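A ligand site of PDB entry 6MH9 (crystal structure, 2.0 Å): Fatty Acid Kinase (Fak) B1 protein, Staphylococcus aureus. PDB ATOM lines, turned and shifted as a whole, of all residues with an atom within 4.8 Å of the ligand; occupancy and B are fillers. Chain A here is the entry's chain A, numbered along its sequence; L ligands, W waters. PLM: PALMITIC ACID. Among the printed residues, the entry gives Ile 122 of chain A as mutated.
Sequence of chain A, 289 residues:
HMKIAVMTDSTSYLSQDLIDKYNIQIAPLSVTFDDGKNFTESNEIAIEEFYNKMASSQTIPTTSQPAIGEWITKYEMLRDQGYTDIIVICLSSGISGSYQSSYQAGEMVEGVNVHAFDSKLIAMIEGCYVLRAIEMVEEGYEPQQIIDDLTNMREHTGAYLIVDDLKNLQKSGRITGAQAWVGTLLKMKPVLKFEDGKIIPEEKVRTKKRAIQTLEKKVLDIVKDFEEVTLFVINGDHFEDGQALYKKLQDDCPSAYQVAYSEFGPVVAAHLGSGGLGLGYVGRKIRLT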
ATOM      1  N   LEU A  29      -9.821  39.498  19.750  1.00  0.00           N
ATOM      2  CA  LEU A  29      -8.555  38.990  20.225  1.00  0.00           C
ATOM      3  C   LEU A  29      -7.758  38.434  19.050  1.00  0.00           C
ATOM      4  O   LEU A  29      -8.262  38.277  17.939  1.00  0.00           O
ATOM      5  CB  LEU A  29      -8.769  37.915  21.297  1.00  0.00           C
ATOM      6  CG  LEU A  29      -9.257  38.374  22.670  1.00  0.00           C
ATOM      7  CD1 LEU A  29     -10.773  38.464  22.710  1.00  0.00           C
ATOM      8  CD2 LEU A  29      -8.752  37.458  23.764  1.00  0.00           C
ATOM      9  N   THR A  63      -1.729  33.944  22.503  1.00  0.00           N
ATOM     10  CA  THR A  63      -2.948  34.728  22.362  1.00  0.00           C
ATOM     11  C   THR A  63      -2.782  36.074  23.060  1.00  0.00           C
ATOM     12  O   THR A  63      -2.042  36.199  24.038  1.00  0.00           O
ATOM     13  CB  THR A  63      -4.150  33.975  22.941  1.00  0.00           C
ATOM     14  OG1 THR A  63      -3.925  33.703  24.328  1.00  0.00           O
ATOM     15  CG2 THR A  63      -4.357  32.661  22.202  1.00  0.00           C
ATOM     16  N   SER A  64      -3.498  37.078  22.554  1.00  0.00           N
ATOM     17  CA  SER A  64      -3.405  38.427  23.062  1.00  0.00           C
ATOM     18  C   SER A  64      -4.803  39.008  23.252  1.00  0.00           C
ATOM     19  O   SER A  64      -5.691  38.792  22.431  1.00  0.00           O
ATOM     20  CB  SER A  64      -2.592  39.324  22.127  1.00  0.00           C
ATOM     21  OG  SER A  64      -1.280  38.819  21.941  1.00  0.00           O
ATOM     22  N   GLN A  65      -4.967  39.746  24.352  1.00  0.00           N
ATOM     23  CA  GLN A  65      -6.212  40.475  24.596  1.00  0.00           C
ATOM     24  C   GLN A  65      -6.382  41.578  23.546  1.00  0.00           C
ATOM     25  O   GLN A  65      -5.435  41.937  22.852  1.00  0.00           O
ATOM     26  CB  GLN A  65      -6.195  41.070  26.001  1.00  0.00           C
ATOM     27  CG  GLN A  65      -5.199  42.213  26.173  1.00  0.00           C
ATOM     28  CD  GLN A  65      -4.660  42.317  27.585  1.00  0.00           C
ATOM     29  OE1 GLN A  65      -5.044  43.202  28.341  1.00  0.00           O
ATOM     30  NE2 GLN A  65      -3.760  41.408  27.941  1.00  0.00           N
ATOM     31  N   LEU A  91     -14.589  37.943  28.396  1.00  0.00           N
ATOM     32  CA  LEU A  91     -14.264  36.622  28.901  1.00  0.00           C
ATOM     33  C   LEU A  91     -13.640  36.738  30.285  1.00  0.00           C
ATOM     34  O   LEU A  91     -13.344  37.825  30.776  1.00  0.00           O
ATOM     35  CB  LEU A  91     -13.330  35.888  27.935  1.00  0.00           C
ATOM     36  CG  LEU A  91     -11.837  36.209  27.976  1.00  0.00           C
ATOM     37  CD1 LEU A  91     -11.038  35.124  27.265  1.00  0.00           C
ATOM     38  CD2 LEU A  91     -11.569  37.550  27.327  1.00  0.00           C
ATOM     39  N   ILE A  95      -8.414  34.363  33.204  1.00  0.00           N
ATOM     40  CA  ILE A  95      -7.673  33.687  32.149  1.00  0.00           C
ATOM     41  C   ILE A  95      -7.231  34.698  31.096  1.00  0.00           C
ATOM     42  O   ILE A  95      -6.478  34.351  30.174  1.00  0.00           O
ATOM     43  CB  ILE A  95      -8.497  32.557  31.501  1.00  0.00           C
ATOM     44  CG1 ILE A  95      -9.699  33.138  30.755  1.00  0.00           C
ATOM     45  CG2 ILE A  95      -8.943  31.545  32.545  1.00  0.00           C
ATOM     46  CD1 ILE A  95     -10.555  32.102  30.063  1.00  0.00           C
ATOM     47  N   SER A  96      -7.684  35.934  31.211  1.00  0.00           N
ATOM     48  CA  SER A  96      -7.372  36.930  30.185  1.00  0.00           C
ATOM     49  C   SER A  96      -7.439  38.330  30.779  1.00  0.00           C
ATOM     50  O   SER A  96      -8.161  38.583  31.745  1.00  0.00           O
ATOM     51  CB  SER A  96      -8.319  36.816  28.988  1.00  0.00           C
ATOM     52  OG  SER A  96      -8.051  37.818  28.036  1.00  0.00           O
ATOM     53  N   GLY A  97      -6.677  39.243  30.173  1.00  0.00           N
ATOM     54  CA  GLY A  97      -6.675  40.639  30.527  1.00  0.00           C
ATOM     55  C   GLY A  97      -7.597  41.510  29.702  1.00  0.00           C
ATOM     56  O   GLY A  97      -7.476  42.735  29.753  1.00  0.00           O
ATOM     57  N   LEU A 121     -16.436  33.343  32.294  1.00  0.00           N
ATOM     58  CA  LEU A 121     -16.481  32.193  31.404  1.00  0.00           C
ATOM     59  C   LEU A 121     -15.951  32.573  30.020  1.00  0.00           C
ATOM     60  O   LEU A 121     -15.148  33.508  29.901  1.00  0.00           O
ATOM     61  CB  LEU A 121     -17.906  31.635  31.290  1.00  0.00           C
ATOM     62  CG  LEU A 121     -18.277  30.325  32.003  1.00  0.00           C
ATOM     63  CD1 LEU A 121     -17.646  29.147  31.281  1.00  0.00           C
ATOM     64  CD2 LEU A 121     -17.927  30.324  33.482  1.00  0.00           C
ATOM     65  N   ILE A 122     -16.393  31.865  28.986  1.00  0.00           N
ATOM     66  CA  ILE A 122     -15.874  32.068  27.644  1.00  0.00           C
ATOM     67  C   ILE A 122     -16.829  31.422  26.640  1.00  0.00           C
ATOM     68  O   ILE A 122     -17.751  30.703  27.012  1.00  0.00           O
ATOM     69  CB  ILE A 122     -14.452  31.486  27.509  1.00  0.00           C
ATOM     70  CG1 ILE A 122     -13.669  32.199  26.405  1.00  0.00           C
ATOM     71  CG2 ILE A 122     -14.506  29.991  27.282  1.00  0.00           C
ATOM     72  CD1 ILE A 122     -12.205  31.812  26.366  1.00  0.00           C
ATOM     73  N   ILE A 125     -21.107  30.615  26.204  1.00  0.00           N
ATOM     74  CA  ILE A 125     -21.555  30.873  27.567  1.00  0.00           C
ATOM     75  C   ILE A 125     -21.369  32.340  27.918  1.00  0.00           C
ATOM     76  O   ILE A 125     -22.262  32.978  28.483  1.00  0.00           O
ATOM     77  CB  ILE A 125     -20.808  29.961  28.564  1.00  0.00           C
ATOM     78  CG1 ILE A 125     -21.107  28.491  28.254  1.00  0.00           C
ATOM     79  CG2 ILE A 125     -21.222  30.288  29.979  1.00  0.00           C
ATOM     80  CD1 ILE A 125     -22.572  28.145  28.325  1.00  0.00           C
ATOM     81  N   ALA A 159     -19.249  25.488  33.408  1.00  0.00           N
ATOM     82  CA  ALA A 159     -18.863  24.695  32.241  1.00  0.00           C
ATOM     83  C   ALA A 159     -17.831  23.659  32.645  1.00  0.00           C
ATOM     84  O   ALA A 159     -16.974  23.927  33.495  1.00  0.00           O
ATOM     85  CB  ALA A 159     -18.293  25.585  31.128  1.00  0.00           C
ATOM     86  N   TYR A 160     -17.927  22.479  32.035  1.00  0.00           N
ATOM     87  CA  TYR A 160     -16.904  21.451  32.100  1.00  0.00           C
ATOM     88  C   TYR A 160     -16.345  21.245  30.691  1.00  0.00           C
ATOM     89  O   TYR A 160     -17.029  21.485  29.700  1.00  0.00           O
ATOM     90  CB  TYR A 160     -17.469  20.129  32.647  1.00  0.00           C
ATOM     91  CG  TYR A 160     -17.924  20.184  34.087  1.00  0.00           C
ATOM     92  CD1 TYR A 160     -19.060  20.893  34.451  1.00  0.00           C
ATOM     93  CD2 TYR A 160     -17.212  19.522  35.085  1.00  0.00           C
ATOM     94  CE1 TYR A 160     -19.478  20.946  35.777  1.00  0.00           C
ATOM     95  CE2 TYR A 160     -17.625  19.564  36.398  1.00  0.00           C
ATOM     96  CZ  TYR A 160     -18.760  20.281  36.739  1.00  0.00           C
ATOM     97  OH  TYR A 160     -19.173  20.323  38.052  1.00  0.00           O
ATOM     98  N   LEU A 161     -15.087  20.800  30.609  1.00  0.00           N
ATOM     99  CA  LEU A 161     -14.448  20.662  29.309  1.00  0.00           C
ATOM    100  C   LEU A 161     -13.493  19.482  29.316  1.00  0.00           C
ATOM    101  O   LEU A 161     -12.971  19.076  30.359  1.00  0.00           O
ATOM    102  CB  LEU A 161     -13.707  21.943  28.911  1.00  0.00           C
ATOM    103  CG  LEU A 161     -12.555  22.387  29.814  1.00  0.00           C
ATOM    104  CD1 LEU A 161     -11.370  22.834  28.969  1.00  0.00           C
ATOM    105  CD2 LEU A 161     -12.993  23.492  30.748  1.00  0.00           C
ATOM    106  N   PHE A 194     -14.743  25.155  34.973  1.00  0.00           N
ATOM    107  CA  PHE A 194     -14.572  26.538  35.386  1.00  0.00           C
ATOM    108  C   PHE A 194     -15.071  26.719  36.805  1.00  0.00           C
ATOM    109  O   PHE A 194     -16.138  26.222  37.176  1.00  0.00           O
ATOM    110  CB  PHE A 194     -15.328  27.476  34.444  1.00  0.00           C
ATOM    111  CG  PHE A 194     -14.527  27.927  33.250  1.00  0.00           C
ATOM    112  CD1 PHE A 194     -14.312  27.066  32.190  1.00  0.00           C
ATOM    113  CD2 PHE A 194     -14.010  29.203  33.184  1.00  0.00           C
ATOM    114  CE1 PHE A 194     -13.580  27.473  31.088  1.00  0.00           C
ATOM    115  CE2 PHE A 194     -13.279  29.621  32.081  1.00  0.00           C
ATOM    116  CZ  PHE A 194     -13.068  28.750  31.035  1.00  0.00           C
ATOM    117  N   ILE A 199      -9.812  27.809  35.562  1.00  0.00           N
ATOM    118  CA  ILE A 199      -9.923  26.442  35.086  1.00  0.00           C
ATOM    119  C   ILE A 199      -9.121  25.548  36.034  1.00  0.00           C
ATOM    120  O   ILE A 199      -7.914  25.757  36.219  1.00  0.00           O
ATOM    121  CB  ILE A 199      -9.426  26.298  33.640  1.00  0.00           C
ATOM    122  CG1 ILE A 199     -10.146  27.293  32.729  1.00  0.00           C
ATOM    123  CG2 ILE A 199      -9.622  24.873  33.144  1.00  0.00           C
ATOM    124  CD1 ILE A 199      -9.613  27.327  31.318  1.00  0.00           C
ATOM    125  N   ILE A 234     -20.163  23.026  23.220  1.00  0.00           N
ATOM    126  CA  ILE A 234     -19.143  23.897  22.627  1.00  0.00           C
ATOM    127  C   ILE A 234     -18.019  22.989  22.132  1.00  0.00           C
ATOM    128  O   ILE A 234     -17.157  22.562  22.907  1.00  0.00           O
ATOM    129  CB  ILE A 234     -18.628  24.947  23.611  1.00  0.00           C
ATOM    130  CG1 ILE A 234     -19.818  25.727  24.176  1.00  0.00           C
ATOM    131  CG2 ILE A 234     -17.635  25.876  22.934  1.00  0.00           C
ATOM    132  CD1 ILE A 234     -19.455  26.998  24.897  1.00  0.00           C
ATOM    133  N   VAL A 267      -8.654  31.404  19.226  1.00  0.00           N
ATOM    134  CA  VAL A 267      -8.045  31.739  20.506  1.00  0.00           C
ATOM    135  C   VAL A 267      -8.228  30.596  21.498  1.00  0.00           C
ATOM    136  O   VAL A 267      -7.280  30.205  22.196  1.00  0.00           O
ATOM    137  CB  VAL A 267      -8.615  33.060  21.048  1.00  0.00           C
ATOM    138  CG1 VAL A 267      -8.426  33.155  22.561  1.00  0.00           C
ATOM    139  CG2 VAL A 267      -7.949  34.240  20.356  1.00  0.00           C
ATOM    140  N   VAL A 268      -9.436  30.034  21.575  1.00  0.00           N
ATOM    141  CA  VAL A 268      -9.679  28.905  22.458  1.00  0.00           C
ATOM    142  C   VAL A 268      -8.970  27.655  21.933  1.00  0.00           C
ATOM    143  O   VAL A 268      -8.415  26.864  22.699  1.00  0.00           O
ATOM    144  CB  VAL A 268     -11.183  28.680  22.639  1.00  0.00           C
ATOM    145  CG1 VAL A 268     -11.446  27.357  23.350  1.00  0.00           C
ATOM    146  CG2 VAL A 268     -11.806  29.834  23.405  1.00  0.00           C
ATOM    147  N   HIS A 271      -5.299  27.193  22.871  1.00  0.00           N
ATOM    148  CA  HIS A 271      -5.011  26.675  24.200  1.00  0.00           C
ATOM    149  C   HIS A 271      -5.501  25.248  24.421  1.00  0.00           C
ATOM    150  O   HIS A 271      -4.925  24.525  25.234  1.00  0.00           O
ATOM    151  CB  HIS A 271      -5.616  27.584  25.271  1.00  0.00           C
ATOM    152  CG  HIS A 271      -4.980  28.936  25.351  1.00  0.00           C
ATOM    153  ND1 HIS A 271      -3.921  29.205  26.188  1.00  0.00           N
ATOM    154  CD2 HIS A 271      -5.252  30.093  24.714  1.00  0.00           C
ATOM    155  CE1 HIS A 271      -3.563  30.474  26.061  1.00  0.00           C
ATOM    156  NE2 HIS A 271      -4.352  31.031  25.158  1.00  0.00           N
ATOM    157  N   LEU A 272      -6.547  24.833  23.709  1.00  0.00           N
ATOM    158  CA  LEU A 272      -7.095  23.497  23.875  1.00  0.00           C
ATOM    159  C   LEU A 272      -6.475  22.483  22.935  1.00  0.00           C
ATOM    160  O   LEU A 272      -6.356  21.304  23.301  1.00  0.00           O
ATOM    161  CB  LEU A 272      -8.617  23.515  23.652  1.00  0.00           C
ATOM    162  CG  LEU A 272      -9.489  23.630  24.893  1.00  0.00           C
ATOM    163  CD1 LEU A 272      -9.464  25.038  25.423  1.00  0.00           C
ATOM    164  CD2 LEU A 272     -10.914  23.200  24.584  1.00  0.00           C
ATOM    165  N   GLY A 278     -16.547  20.908  25.180  1.00  0.00           N
ATOM    166  CA  GLY A 278     -17.033  21.376  26.462  1.00  0.00           C
ATOM    167  C   GLY A 278     -18.547  21.386  26.502  1.00  0.00           C
ATOM    168  O   GLY A 278     -19.223  21.340  25.472  1.00  0.00           O
ATOM    169  N   LEU A 279     -19.065  21.441  27.727  1.00  0.00           N
ATOM    170  CA  LEU A 279     -20.500  21.541  27.972  1.00  0.00           C
ATOM    171  C   LEU A 279     -20.726  22.650  28.989  1.00  0.00           C
ATOM    172  O   LEU A 279     -20.318  22.523  30.152  1.00  0.00           O
ATOM    173  CB  LEU A 279     -21.076  20.213  28.470  1.00  0.00           C
ATOM    174  CG  LEU A 279     -22.563  20.222  28.818  1.00  0.00           C
ATOM    175  CD1 LEU A 279     -23.385  20.818  27.669  1.00  0.00           C
ATOM    176  CD2 LEU A 279     -23.047  18.819  29.153  1.00  0.00           C
ATOM    177  N   GLY A 280     -21.365  23.728  28.559  1.00  0.00           N
ATOM    178  CA  GLY A 280     -21.684  24.834  29.441  1.00  0.00           C
ATOM    179  C   GLY A 280     -23.151  24.884  29.785  1.00  0.00           C
ATOM    180  O   GLY A 280     -23.979  24.303  29.090  1.00  0.00           O
HETATM  181  C1  PLM L   1      -5.758  36.307  26.120  1.00  0.00           C
HETATM  182  O1  PLM L   1      -4.691  36.109  25.511  1.00  0.00           O
HETATM  183  O2  PLM L   1      -6.020  37.275  26.831  1.00  0.00           O
HETATM  184  C2  PLM L   1      -6.896  35.206  25.949  1.00  0.00           C
HETATM  185  C3  PLM L   1      -6.625  33.914  26.728  1.00  0.00           C
HETATM  186  C4  PLM L   1      -7.630  32.759  26.462  1.00  0.00           C
HETATM  187  C5  PLM L   1      -7.346  31.459  27.247  1.00  0.00           C
HETATM  188  C6  PLM L   1      -8.307  30.273  26.956  1.00  0.00           C
HETATM  189  C7  PLM L   1      -8.192  29.089  27.953  1.00  0.00           C
HETATM  190  C8  PLM L   1      -9.076  27.854  27.635  1.00  0.00           C
HETATM  191  C9  PLM L   1     -10.605  28.099  27.624  1.00  0.00           C
HETATM  192  CA  PLM L   1     -11.490  26.823  27.798  1.00  0.00           C
HETATM  193  CB  PLM L   1     -12.878  26.884  27.112  1.00  0.00           C
HETATM  194  CC  PLM L   1     -13.563  25.517  26.847  1.00  0.00           C
HETATM  195  CD  PLM L   1     -15.099  25.580  26.667  1.00  0.00           C
HETATM  196  CE  PLM L   1     -15.861  26.135  27.894  1.00  0.00           C
HETATM  197  CF  PLM L   1     -17.386  26.229  27.716  1.00  0.00           C
HETATM  198  CG  PLM L   1     -18.033  24.854  27.534  1.00  0.00           C
HETATM  199  O   HOH W   1      -2.334  37.477  26.659  1.00  0.00           O
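O2 of the ligand lies within hydrogen-bond range of OG of Ser 96 (2.4 Å). O of Thr 63 sits close to O1 of the ligand, 3.0 Å away. The side-chain hydroxyl (OG1) of Thr 63 sits at hydrogen-bond distance from an oxygen (O1) of the ligand, 2.8 Å away. N of Ser 64 sits at hydrogen-bond distance from O1 of the ligand.
OG1 of Thr 63 lies within hydrogen-bond range of NE2 of His 271 (2.8 Å). N of Leu 279 sits at hydrogen-bond distance from O of Tyr 160 (2.8 Å). The backbone carbonyl oxygen (O) of Ile 234 lies within hydrogen-bond range of the backbone NH (N) of Gly 278, at 2.9 Å. The backbone carbonyl oxygen (O) of Ala 159 lies within hydrogen-bond range of the backbone NH (N) of Phe 194 (2.9 Å). OE1 of Gln 65 lies close to O of Gly 97 (2.9 Å).
Residues that only touch the ligand: Leu 29, Gln 65, Ile 95, Gly 97, Ile 122, Ala 159, Phe 194, Ile 199, Ile 234, His 271, Leu 272, Gly 278, Leu 279 and Gly 280. Hydrophobic or aromatic side chains that line the ligand: Leu 29, Ile 122, Ala 159, Phe 194, Ile 199, Ile 234, His 271 and Leu 272. 17 residues have an atom within 4 Å of the ligand: Leu 29, Thr 63, Ser 64, Gln 65, Ile 95, Ser 96, Gly 97, Ile 122, Ala 159, Phe 194, Ile 199, Ile 234, His 271, Leu 272, Gly 278, Leu 279 and Gly 280. The nearest printed residue that does not touch the ligand is Val 267 (4.001 Å).
Water W1 lies within hydrogen-bond range of O of Thr 63 and O1 of the ligand.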
